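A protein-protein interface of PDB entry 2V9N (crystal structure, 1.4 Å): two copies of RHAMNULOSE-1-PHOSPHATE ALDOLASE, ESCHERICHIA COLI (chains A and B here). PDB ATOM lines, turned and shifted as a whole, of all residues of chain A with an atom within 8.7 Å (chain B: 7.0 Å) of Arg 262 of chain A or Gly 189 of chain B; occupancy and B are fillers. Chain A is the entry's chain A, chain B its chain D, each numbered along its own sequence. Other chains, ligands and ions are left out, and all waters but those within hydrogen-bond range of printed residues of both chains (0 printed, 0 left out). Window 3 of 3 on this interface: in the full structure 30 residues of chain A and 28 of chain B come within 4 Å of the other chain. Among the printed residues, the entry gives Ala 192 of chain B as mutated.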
ATOM      1  N   THR A 170      -8.343   8.420  10.059  1.00  0.00           N
ATOM      2  CA  THR A 170      -8.501   9.025   8.732  1.00  0.00           C
ATOM      3  C   THR A 170      -8.287  10.542   8.722  1.00  0.00           C
ATOM      4  O   THR A 170      -7.686  11.074   7.797  1.00  0.00           O
ATOM      5  CB  THR A 170      -9.870   8.623   8.120  1.00  0.00           C
ATOM      6  OG1 THR A 170      -9.812   7.240   7.740  1.00  0.00           O
ATOM      7  CG2 THR A 170     -10.238   9.465   6.887  1.00  0.00           C
ATOM      8  N   LEU A 173      -4.351  13.208   8.226  1.00  0.00           N
ATOM      9  CA  LEU A 173      -3.733  13.898   7.096  1.00  0.00           C
ATOM     10  C   LEU A 173      -4.337  15.292   6.903  1.00  0.00           C
ATOM     11  O   LEU A 173      -3.639  16.209   6.481  1.00  0.00           O
ATOM     12  CB  LEU A 173      -3.830  13.053   5.819  1.00  0.00           C
ATOM     13  CG  LEU A 173      -3.259  13.676   4.543  1.00  0.00           C
ATOM     14  CD1 LEU A 173      -2.573  12.601   3.726  1.00  0.00           C
ATOM     15  CD2 LEU A 173      -4.357  14.359   3.739  1.00  0.00           C
ATOM     16  N   VAL A 174      -5.618  15.459   7.232  1.00  0.00           N
ATOM     17  CA  VAL A 174      -6.273  16.764   7.086  1.00  0.00           C
ATOM     18  C   VAL A 174      -5.935  17.693   8.260  1.00  0.00           C
ATOM     19  O   VAL A 174      -5.753  18.902   8.057  1.00  0.00           O
ATOM     20  CB  VAL A 174      -7.789  16.609   6.944  1.00  0.00           C
ATOM     21  CG1 VAL A 174      -8.447  17.968   6.683  1.00  0.00           C
ATOM     22  CG2 VAL A 174      -8.097  15.639   5.821  1.00  0.00           C
ATOM     23  N   GLU A 255      -5.384   6.339  -1.216  1.00  0.00           N
ATOM     24  CA  GLU A 255      -6.443   6.875  -0.355  1.00  0.00           C
ATOM     25  C   GLU A 255      -6.005   8.185   0.319  1.00  0.00           C
ATOM     26  O   GLU A 255      -6.761   9.155   0.344  1.00  0.00           O
ATOM     27  CB  GLU A 255      -6.894   5.820   0.670  1.00  0.00           C
ATOM     28  CG  GLU A 255      -7.666   4.660   0.010  1.00  0.00           C
ATOM     29  CD  GLU A 255      -7.844   3.424   0.883  1.00  0.00           C
ATOM     30  OE1 GLU A 255      -8.740   2.610   0.549  1.00  0.00           O
ATOM     31  OE2 GLU A 255      -7.108   3.248   1.882  1.00  0.00           O
ATOM     32  N   LEU A 256      -4.772   8.236   0.821  1.00  0.00           N
ATOM     33  CA  LEU A 256      -4.230   9.487   1.374  1.00  0.00           C
ATOM     34  C   LEU A 256      -4.202  10.610   0.329  1.00  0.00           C
ATOM     35  O   LEU A 256      -4.528  11.762   0.631  1.00  0.00           O
ATOM     36  CB  LEU A 256      -2.824   9.269   1.942  1.00  0.00           C
ATOM     37  CG  LEU A 256      -2.770   8.367   3.185  1.00  0.00           C
ATOM     38  CD1 LEU A 256      -1.324   8.020   3.510  1.00  0.00           C
ATOM     39  CD2 LEU A 256      -3.444   9.015   4.383  1.00  0.00           C
ATOM     40  N   ILE A 257      -3.826  10.272  -0.903  1.00  0.00           N
ATOM     41  CA  ILE A 257      -3.794  11.263  -1.982  1.00  0.00           C
ATOM     42  C   ILE A 257      -5.205  11.805  -2.255  1.00  0.00           C
ATOM     43  O   ILE A 257      -5.399  13.023  -2.339  1.00  0.00           O
ATOM     44  CB  ILE A 257      -3.153  10.691  -3.270  1.00  0.00           C
ATOM     45  CG1 ILE A 257      -1.656  10.474  -3.043  1.00  0.00           C
ATOM     46  CG2 ILE A 257      -3.333  11.641  -4.457  1.00  0.00           C
ATOM     47  CD1 ILE A 257      -0.957   9.784  -4.207  1.00  0.00           C
ATOM     48  N   ALA A 258      -6.183  10.903  -2.342  1.00  0.00           N
ATOM     49  CA  ALA A 258      -7.588  11.288  -2.554  1.00  0.00           C
ATOM     50  C   ALA A 258      -8.141  12.154  -1.416  1.00  0.00           C
ATOM     51  O   ALA A 258      -8.893  13.113  -1.635  1.00  0.00           O
ATOM     52  CB  ALA A 258      -8.453  10.044  -2.742  1.00  0.00           C
ATOM     53  N   LEU A 259      -7.762  11.802  -0.193  1.00  0.00           N
ATOM     54  CA  LEU A 259      -8.149  12.568   0.981  1.00  0.00           C
ATOM     55  C   LEU A 259      -7.589  14.002   0.916  1.00  0.00           C
ATOM     56  O   LEU A 259      -8.320  14.975   1.134  1.00  0.00           O
ATOM     57  CB  LEU A 259      -7.643  11.843   2.221  1.00  0.00           C
ATOM     58  CG  LEU A 259      -8.007  12.393   3.586  1.00  0.00           C
ATOM     59  CD1 LEU A 259      -9.512  12.365   3.813  1.00  0.00           C
ATOM     60  CD2 LEU A 259      -7.277  11.526   4.600  1.00  0.00           C
ATOM     61  N   GLY A 260      -6.305  14.123   0.601  1.00  0.00           N
ATOM     62  CA  GLY A 260      -5.656  15.417   0.486  1.00  0.00           C
ATOM     63  C   GLY A 260      -6.294  16.270  -0.596  1.00  0.00           C
ATOM     64  O   GLY A 260      -6.529  17.458  -0.397  1.00  0.00           O
ATOM     65  N   LYS A 261      -6.582  15.645  -1.738  1.00  0.00           N
ATOM     66  CA  LYS A 261      -7.302  16.322  -2.839  1.00  0.00           C
ATOM     67  C   LYS A 261      -8.639  16.912  -2.358  1.00  0.00           C
ATOM     68  O   LYS A 261      -8.923  18.103  -2.545  1.00  0.00           O
ATOM     69  CB  LYS A 261      -7.553  15.379  -4.023  1.00  0.00           C
ATOM     70  CG  LYS A 261      -8.239  16.085  -5.201  1.00  0.00           C
ATOM     71  CD  LYS A 261      -8.120  15.311  -6.507  1.00  0.00           C
ATOM     72  CE  LYS A 261      -8.648  16.130  -7.684  1.00  0.00           C
ATOM     73  NZ  LYS A 261      -8.834  15.302  -8.912  1.00  0.00           N
ATOM     74  N   ARG A 262      -9.459  16.066  -1.744  1.00  0.00           N
ATOM     75  CA  ARG A 262     -10.796  16.472  -1.320  1.00  0.00           C
ATOM     76  C   ARG A 262     -10.765  17.692  -0.405  1.00  0.00           C
ATOM     77  O   ARG A 262     -11.576  18.599  -0.557  1.00  0.00           O
ATOM     78  CB  ARG A 262     -11.515  15.310  -0.620  1.00  0.00           C
ATOM     79  CG  ARG A 262     -12.876  15.666  -0.004  1.00  0.00           C
ATOM     80  CD  ARG A 262     -13.813  16.277  -1.030  1.00  0.00           C
ATOM     81  NE  ARG A 262     -15.162  16.511  -0.522  1.00  0.00           N
ATOM     82  CZ  ARG A 262     -15.510  17.478   0.330  1.00  0.00           C
ATOM     83  NH1 ARG A 262     -16.779  17.590   0.689  1.00  0.00           N
ATOM     84  NH2 ARG A 262     -14.620  18.323   0.843  1.00  0.00           N
ATOM     85  N   PHE A 263      -9.818  17.710   0.527  1.00  0.00           N
ATOM     86  CA  PHE A 263      -9.760  18.749   1.554  1.00  0.00           C
ATOM     87  C   PHE A 263      -8.754  19.858   1.246  1.00  0.00           C
ATOM     88  O   PHE A 263      -8.508  20.734   2.080  1.00  0.00           O
ATOM     89  CB  PHE A 263      -9.527  18.094   2.929  1.00  0.00           C
ATOM     90  CG  PHE A 263     -10.717  17.311   3.405  1.00  0.00           C
ATOM     91  CD1 PHE A 263     -10.777  15.926   3.269  1.00  0.00           C
ATOM     92  CD2 PHE A 263     -11.824  17.975   3.917  1.00  0.00           C
ATOM     93  CE1 PHE A 263     -11.911  15.222   3.685  1.00  0.00           C
ATOM     94  CE2 PHE A 263     -12.941  17.280   4.322  1.00  0.00           C
ATOM     95  CZ  PHE A 263     -12.988  15.903   4.213  1.00  0.00           C
ATOM     96  N   GLY A 264      -8.203  19.838   0.034  1.00  0.00           N
ATOM     97  CA  GLY A 264      -7.322  20.908  -0.430  1.00  0.00           C
ATOM     98  C   GLY A 264      -6.075  21.117   0.407  1.00  0.00           C
ATOM     99  O   GLY A 264      -5.659  22.252   0.628  1.00  0.00           O
ATOM    100  N   VAL A 265      -5.472  20.024   0.859  1.00  0.00           N
ATOM    101  CA  VAL A 265      -4.227  20.098   1.621  1.00  0.00           C
ATOM    102  C   VAL A 265      -3.134  19.387   0.855  1.00  0.00           C
ATOM    103  O   VAL A 265      -3.410  18.459   0.090  1.00  0.00           O
ATOM    104  CB  VAL A 265      -4.365  19.491   3.052  1.00  0.00           C
ATOM    105  CG1 VAL A 265      -5.310  20.323   3.880  1.00  0.00           C
ATOM    106  CG2 VAL A 265      -4.803  18.013   3.025  1.00  0.00           C
ATOM    107  N   SER B 116     -20.269  18.701   8.494  1.00  0.00           N
ATOM    108  CA  SER B 116     -19.883  18.383   7.130  1.00  0.00           C
ATOM    109  C   SER B 116     -20.226  16.937   6.743  1.00  0.00           C
ATOM    110  O   SER B 116     -20.102  16.580   5.573  1.00  0.00           O
ATOM    111  CB  SER B 116     -18.388  18.646   6.936  1.00  0.00           C
ATOM    112  OG  SER B 116     -17.610  17.735   7.680  1.00  0.00           O
ATOM    113  N   GLU B 117     -20.625  16.102   7.708  1.00  0.00           N
ATOM    114  CA  GLU B 117     -21.175  14.784   7.407  1.00  0.00           C
ATOM    115  C   GLU B 117     -22.705  14.805   7.339  1.00  0.00           C
ATOM    116  O   GLU B 117     -23.343  13.779   7.498  1.00  0.00           O
ATOM    117  CB  GLU B 117     -20.706  13.749   8.436  1.00  0.00           C
ATOM    118  CG  GLU B 117     -19.195  13.493   8.415  1.00  0.00           C
ATOM    119  CD  GLU B 117     -18.684  12.877   7.115  1.00  0.00           C
ATOM    120  OE1 GLU B 117     -17.443  12.724   6.962  1.00  0.00           O
ATOM    121  OE2 GLU B 117     -19.512  12.527   6.246  1.00  0.00           O
ATOM    122  N   LEU B 118     -23.300  15.969   7.078  1.00  0.00           N
ATOM    123  CA  LEU B 118     -24.760  16.067   6.964  1.00  0.00           C
ATOM    124  C   LEU B 118     -25.353  15.101   5.917  1.00  0.00           C
ATOM    125  O   LEU B 118     -26.417  14.535   6.157  1.00  0.00           O
ATOM    126  CB  LEU B 118     -25.217  17.514   6.693  1.00  0.00           C
ATOM    127  CG  LEU B 118     -26.682  17.815   7.028  1.00  0.00           C
ATOM    128  CD1 LEU B 118     -26.931  17.697   8.528  1.00  0.00           C
ATOM    129  CD2 LEU B 118     -27.099  19.188   6.526  1.00  0.00           C
ATOM    130  N   PRO B 119     -24.690  14.908   4.759  1.00  0.00           N
ATOM    131  CA  PRO B 119     -25.259  13.908   3.855  1.00  0.00           C
ATOM    132  C   PRO B 119     -25.389  12.525   4.511  1.00  0.00           C
ATOM    133  O   PRO B 119     -26.447  11.912   4.438  1.00  0.00           O
ATOM    134  CB  PRO B 119     -24.270  13.901   2.670  1.00  0.00           C
ATOM    135  CG  PRO B 119     -23.636  15.235   2.705  1.00  0.00           C
ATOM    136  CD  PRO B 119     -23.505  15.563   4.177  1.00  0.00           C
ATOM    137  N   MET B 186     -13.614   5.083   2.527  1.00  0.00           N
ATOM    138  CA  MET B 186     -14.134   6.076   1.587  1.00  0.00           C
ATOM    139  C   MET B 186     -13.779   7.482   2.055  1.00  0.00           C
ATOM    140  O   MET B 186     -13.571   7.723   3.242  1.00  0.00           O
ATOM    141  CB  MET B 186     -15.659   5.941   1.444  1.00  0.00           C
ATOM    142  CG  MET B 186     -16.097   4.633   0.806  1.00  0.00           C
ATOM    143  SD  MET B 186     -17.884   4.380   0.638  1.00  0.00           S
ATOM    144  CE  MET B 186     -18.286   5.604  -0.613  1.00  0.00           C
ATOM    145  N   VAL B 187     -13.715   8.415   1.115  1.00  0.00           N
ATOM    146  CA  VAL B 187     -13.366   9.792   1.437  1.00  0.00           C
ATOM    147  C   VAL B 187     -14.459  10.421   2.316  1.00  0.00           C
ATOM    148  O   VAL B 187     -15.642  10.429   1.948  1.00  0.00           O
ATOM    149  CB  VAL B 187     -13.143  10.640   0.170  1.00  0.00           C
ATOM    150  CG1 VAL B 187     -12.747  12.051   0.558  1.00  0.00           C
ATOM    151  CG2 VAL B 187     -12.079   9.999  -0.713  1.00  0.00           C
ATOM    152  N   PRO B 188     -14.078  10.938   3.495  1.00  0.00           N
ATOM    153  CA  PRO B 188     -15.084  11.581   4.352  1.00  0.00           C
ATOM    154  C   PRO B 188     -15.744  12.821   3.750  1.00  0.00           C
ATOM    155  O   PRO B 188     -15.149  13.516   2.922  1.00  0.00           O
ATOM    156  CB  PRO B 188     -14.283  11.986   5.594  1.00  0.00           C
ATOM    157  CG  PRO B 188     -13.065  11.179   5.565  1.00  0.00           C
ATOM    158  CD  PRO B 188     -12.745  10.945   4.125  1.00  0.00           C
ATOM    159  N   GLY B 189     -16.970  13.094   4.178  1.00  0.00           N
ATOM    160  CA  GLY B 189     -17.635  14.353   3.864  1.00  0.00           C
ATOM    161  C   GLY B 189     -18.175  14.439   2.454  1.00  0.00           C
ATOM    162  O   GLY B 189     -18.450  15.537   1.958  1.00  0.00           O
ATOM    163  N   THR B 190     -18.346  13.285   1.821  1.00  0.00           N
ATOM    164  CA  THR B 190     -18.829  13.214   0.450  1.00  0.00           C
ATOM    165  C   THR B 190     -20.253  12.695   0.415  1.00  0.00           C
ATOM    166  O   THR B 190     -20.716  12.061   1.362  1.00  0.00           O
ATOM    167  CB  THR B 190     -17.955  12.259  -0.392  1.00  0.00           C
ATOM    168  OG1 THR B 190     -17.941  10.951   0.200  1.00  0.00           O
ATOM    169  CG2 THR B 190     -16.532  12.773  -0.504  1.00  0.00           C
ATOM    170  N   ASP B 191     -21.000  12.939  -0.666  1.00  0.00           N
ATOM    171  CA  ASP B 191     -22.295  12.265  -0.782  1.00  0.00           C
ATOM    172  C   ASP B 191     -22.097  10.770  -1.018  1.00  0.00           C
ATOM    173  O   ASP B 191     -22.958   9.974  -0.648  1.00  0.00           O
ATOM    174  CB  ASP B 191     -23.169  12.838  -1.895  1.00  0.00           C
ATOM    175  CG  ASP B 191     -23.798  14.162  -1.523  1.00  0.00           C
ATOM    176  OD1 ASP B 191     -23.220  15.196  -1.909  1.00  0.00           O
ATOM    177  OD2 ASP B 191     -24.865  14.172  -0.863  1.00  0.00           O
ATOM    178  N   ALA B 192     -20.976  10.374  -1.629  1.00  0.00           N
ATOM    179  CA  ALA B 192     -20.732   8.945  -1.807  1.00  0.00           C
ATOM    180  C   ALA B 192     -20.721   8.192  -0.474  1.00  0.00           C
ATOM    181  O   ALA B 192     -21.413   7.198  -0.317  1.00  0.00           O
ATOM    182  CB  ALA B 192     -19.425   8.706  -2.556  1.00  0.00           C
ATOM    183  N   ILE B 193     -19.936   8.672   0.483  1.00  0.00           N
ATOM    184  CA  ILE B 193     -19.839   7.986   1.772  1.00  0.00           C
ATOM    185  C   ILE B 193     -21.166   8.099   2.529  1.00  0.00           C
ATOM    186  O   ILE B 193     -21.565   7.177   3.236  1.00  0.00           O
ATOM    187  CB  ILE B 193     -18.635   8.476   2.626  1.00  0.00           C
ATOM    188  CG1 ILE B 193     -18.269   7.420   3.685  1.00  0.00           C
ATOM    189  CG2 ILE B 193     -18.919   9.823   3.288  1.00  0.00           C
ATOM    190  CD1 ILE B 193     -16.952   7.706   4.421  1.00  0.00           C
ATOM    191  N   GLY B 194     -21.852   9.228   2.356  1.00  0.00           N
ATOM    192  CA  GLY B 194     -23.159   9.426   2.962  1.00  0.00           C
ATOM    193  C   GLY B 194     -24.218   8.473   2.449  1.00  0.00           C
ATOM    194  O   GLY B 194     -24.945   7.866   3.231  1.00  0.00           O
ATOM    195  N   TRP B 209     -16.851   2.553   9.373  1.00  0.00           N
ATOM    196  CA  TRP B 209     -15.991   3.221   8.412  1.00  0.00           C
ATOM    197  C   TRP B 209     -14.573   2.787   8.762  1.00  0.00           C
ATOM    198  O   TRP B 209     -14.017   3.254   9.763  1.00  0.00           O
ATOM    199  CB  TRP B 209     -16.127   4.734   8.591  1.00  0.00           C
ATOM    200  CG  TRP B 209     -17.391   5.308   8.003  1.00  0.00           C
ATOM    201  CD1 TRP B 209     -18.462   4.618   7.504  1.00  0.00           C
ATOM    202  CD2 TRP B 209     -17.711   6.698   7.869  1.00  0.00           C
ATOM    203  NE1 TRP B 209     -19.415   5.499   7.045  1.00  0.00           N
ATOM    204  CE2 TRP B 209     -18.981   6.780   7.263  1.00  0.00           C
ATOM    205  CE3 TRP B 209     -17.045   7.882   8.200  1.00  0.00           C
ATOM    206  CZ2 TRP B 209     -19.591   8.002   6.962  1.00  0.00           C
ATOM    207  CZ3 TRP B 209     -17.657   9.102   7.908  1.00  0.00           C
ATOM    208  CH2 TRP B 209     -18.915   9.146   7.283  1.00  0.00           C
ATOM    209  N   HIS B 212     -11.456   4.725  10.691  1.00  0.00           N
ATOM    210  CA  HIS B 212     -12.154   5.993  10.916  1.00  0.00           C
ATOM    211  C   HIS B 212     -13.132   5.929  12.103  1.00  0.00           C
ATOM    212  O   HIS B 212     -12.915   6.588  13.112  1.00  0.00           O
ATOM    213  CB  HIS B 212     -12.861   6.450   9.630  1.00  0.00           C
ATOM    214  CG  HIS B 212     -13.519   7.794   9.743  1.00  0.00           C
ATOM    215  ND1 HIS B 212     -13.794   8.580   8.642  1.00  0.00           N
ATOM    216  CD2 HIS B 212     -13.922   8.508  10.821  1.00  0.00           C
ATOM    217  CE1 HIS B 212     -14.369   9.704   9.043  1.00  0.00           C
ATOM    218  NE2 HIS B 212     -14.462   9.682  10.361  1.00  0.00           N
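The guanidinium group of Arg 262 of chain A lies within hydrogen-bond range of the backbone carbonyl oxygen of Gly 189 of chain B (2.9 Å).
The side-chain carboxylate (OE1) of Glu 117 of chain B is in hydrogen-bond range of the backbone NH (N) of Gly 189 of chain B (2.8 Å).
The backbone carbonyl oxygen (O) of Val 187 of chain B is in hydrogen-bond range of the side-chain hydroxyl (OG1) of Thr 190 of chain B (2.9 Å).
The side-chain hydroxyl (OG1) of Thr 190 of chain B sits at hydrogen-bond distance from the backbone NH (N) of Ile 193 of chain B (3.0 Å).
Among the printed residues, pairs that only touch across the chains: Thr 170 of chain A with Pro 188 of chain B, Thr 170 of chain A with His 212 of chain B, Leu 259 of chain A with Pro 188 of chain B, Arg 262 of chain A with Val 187 of chain B, Arg 262 of chain A with Thr 190 of chain B and Phe 263 of chain A with Pro 188 of chain B.
Of the printed residues of chain B, Leu 259 of chain A touches Pro 188.
Printed residues of chain B within 4 Å of Arg 262 of chain A: Val 187 (3.7 Å), Gly 189 (2.9 Å) and Thr 190 (3.98 Å).
Of the printed residues of chain A, Pro 188 of chain B touches Thr 170 (3.6 Å), Leu 259 (3.5 Å) and Phe 263 (3.5 Å).
Of the printed residues of chain A, Gly 189 of chain B touches Arg 262.
Asp 191 of chain B touches none of the printed residues of chain A.
The nearest printed residue of chain B that does not touch Arg 262 of chain A is Pro 188 of chain B (4.3 Å).
Of the 15 printed residues of chain B, 5 touch a printed residue of chain A.
Printed residues of chain B that touch a printed residue of chain A: Val 187, Pro 188, Gly 189, Thr 190 and His 212.
Of the 14 printed residues of chain A, 4 touch a printed residue of chain B.
Hydrophobic or aromatic side chains of chain A that line the printed part of chain B: Leu 259 and Phe 263.
No position is printed for both chains.
Of the 7 pairs that touch across the chains among the printed residues, none has its exchanged pair printed and touching as well.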
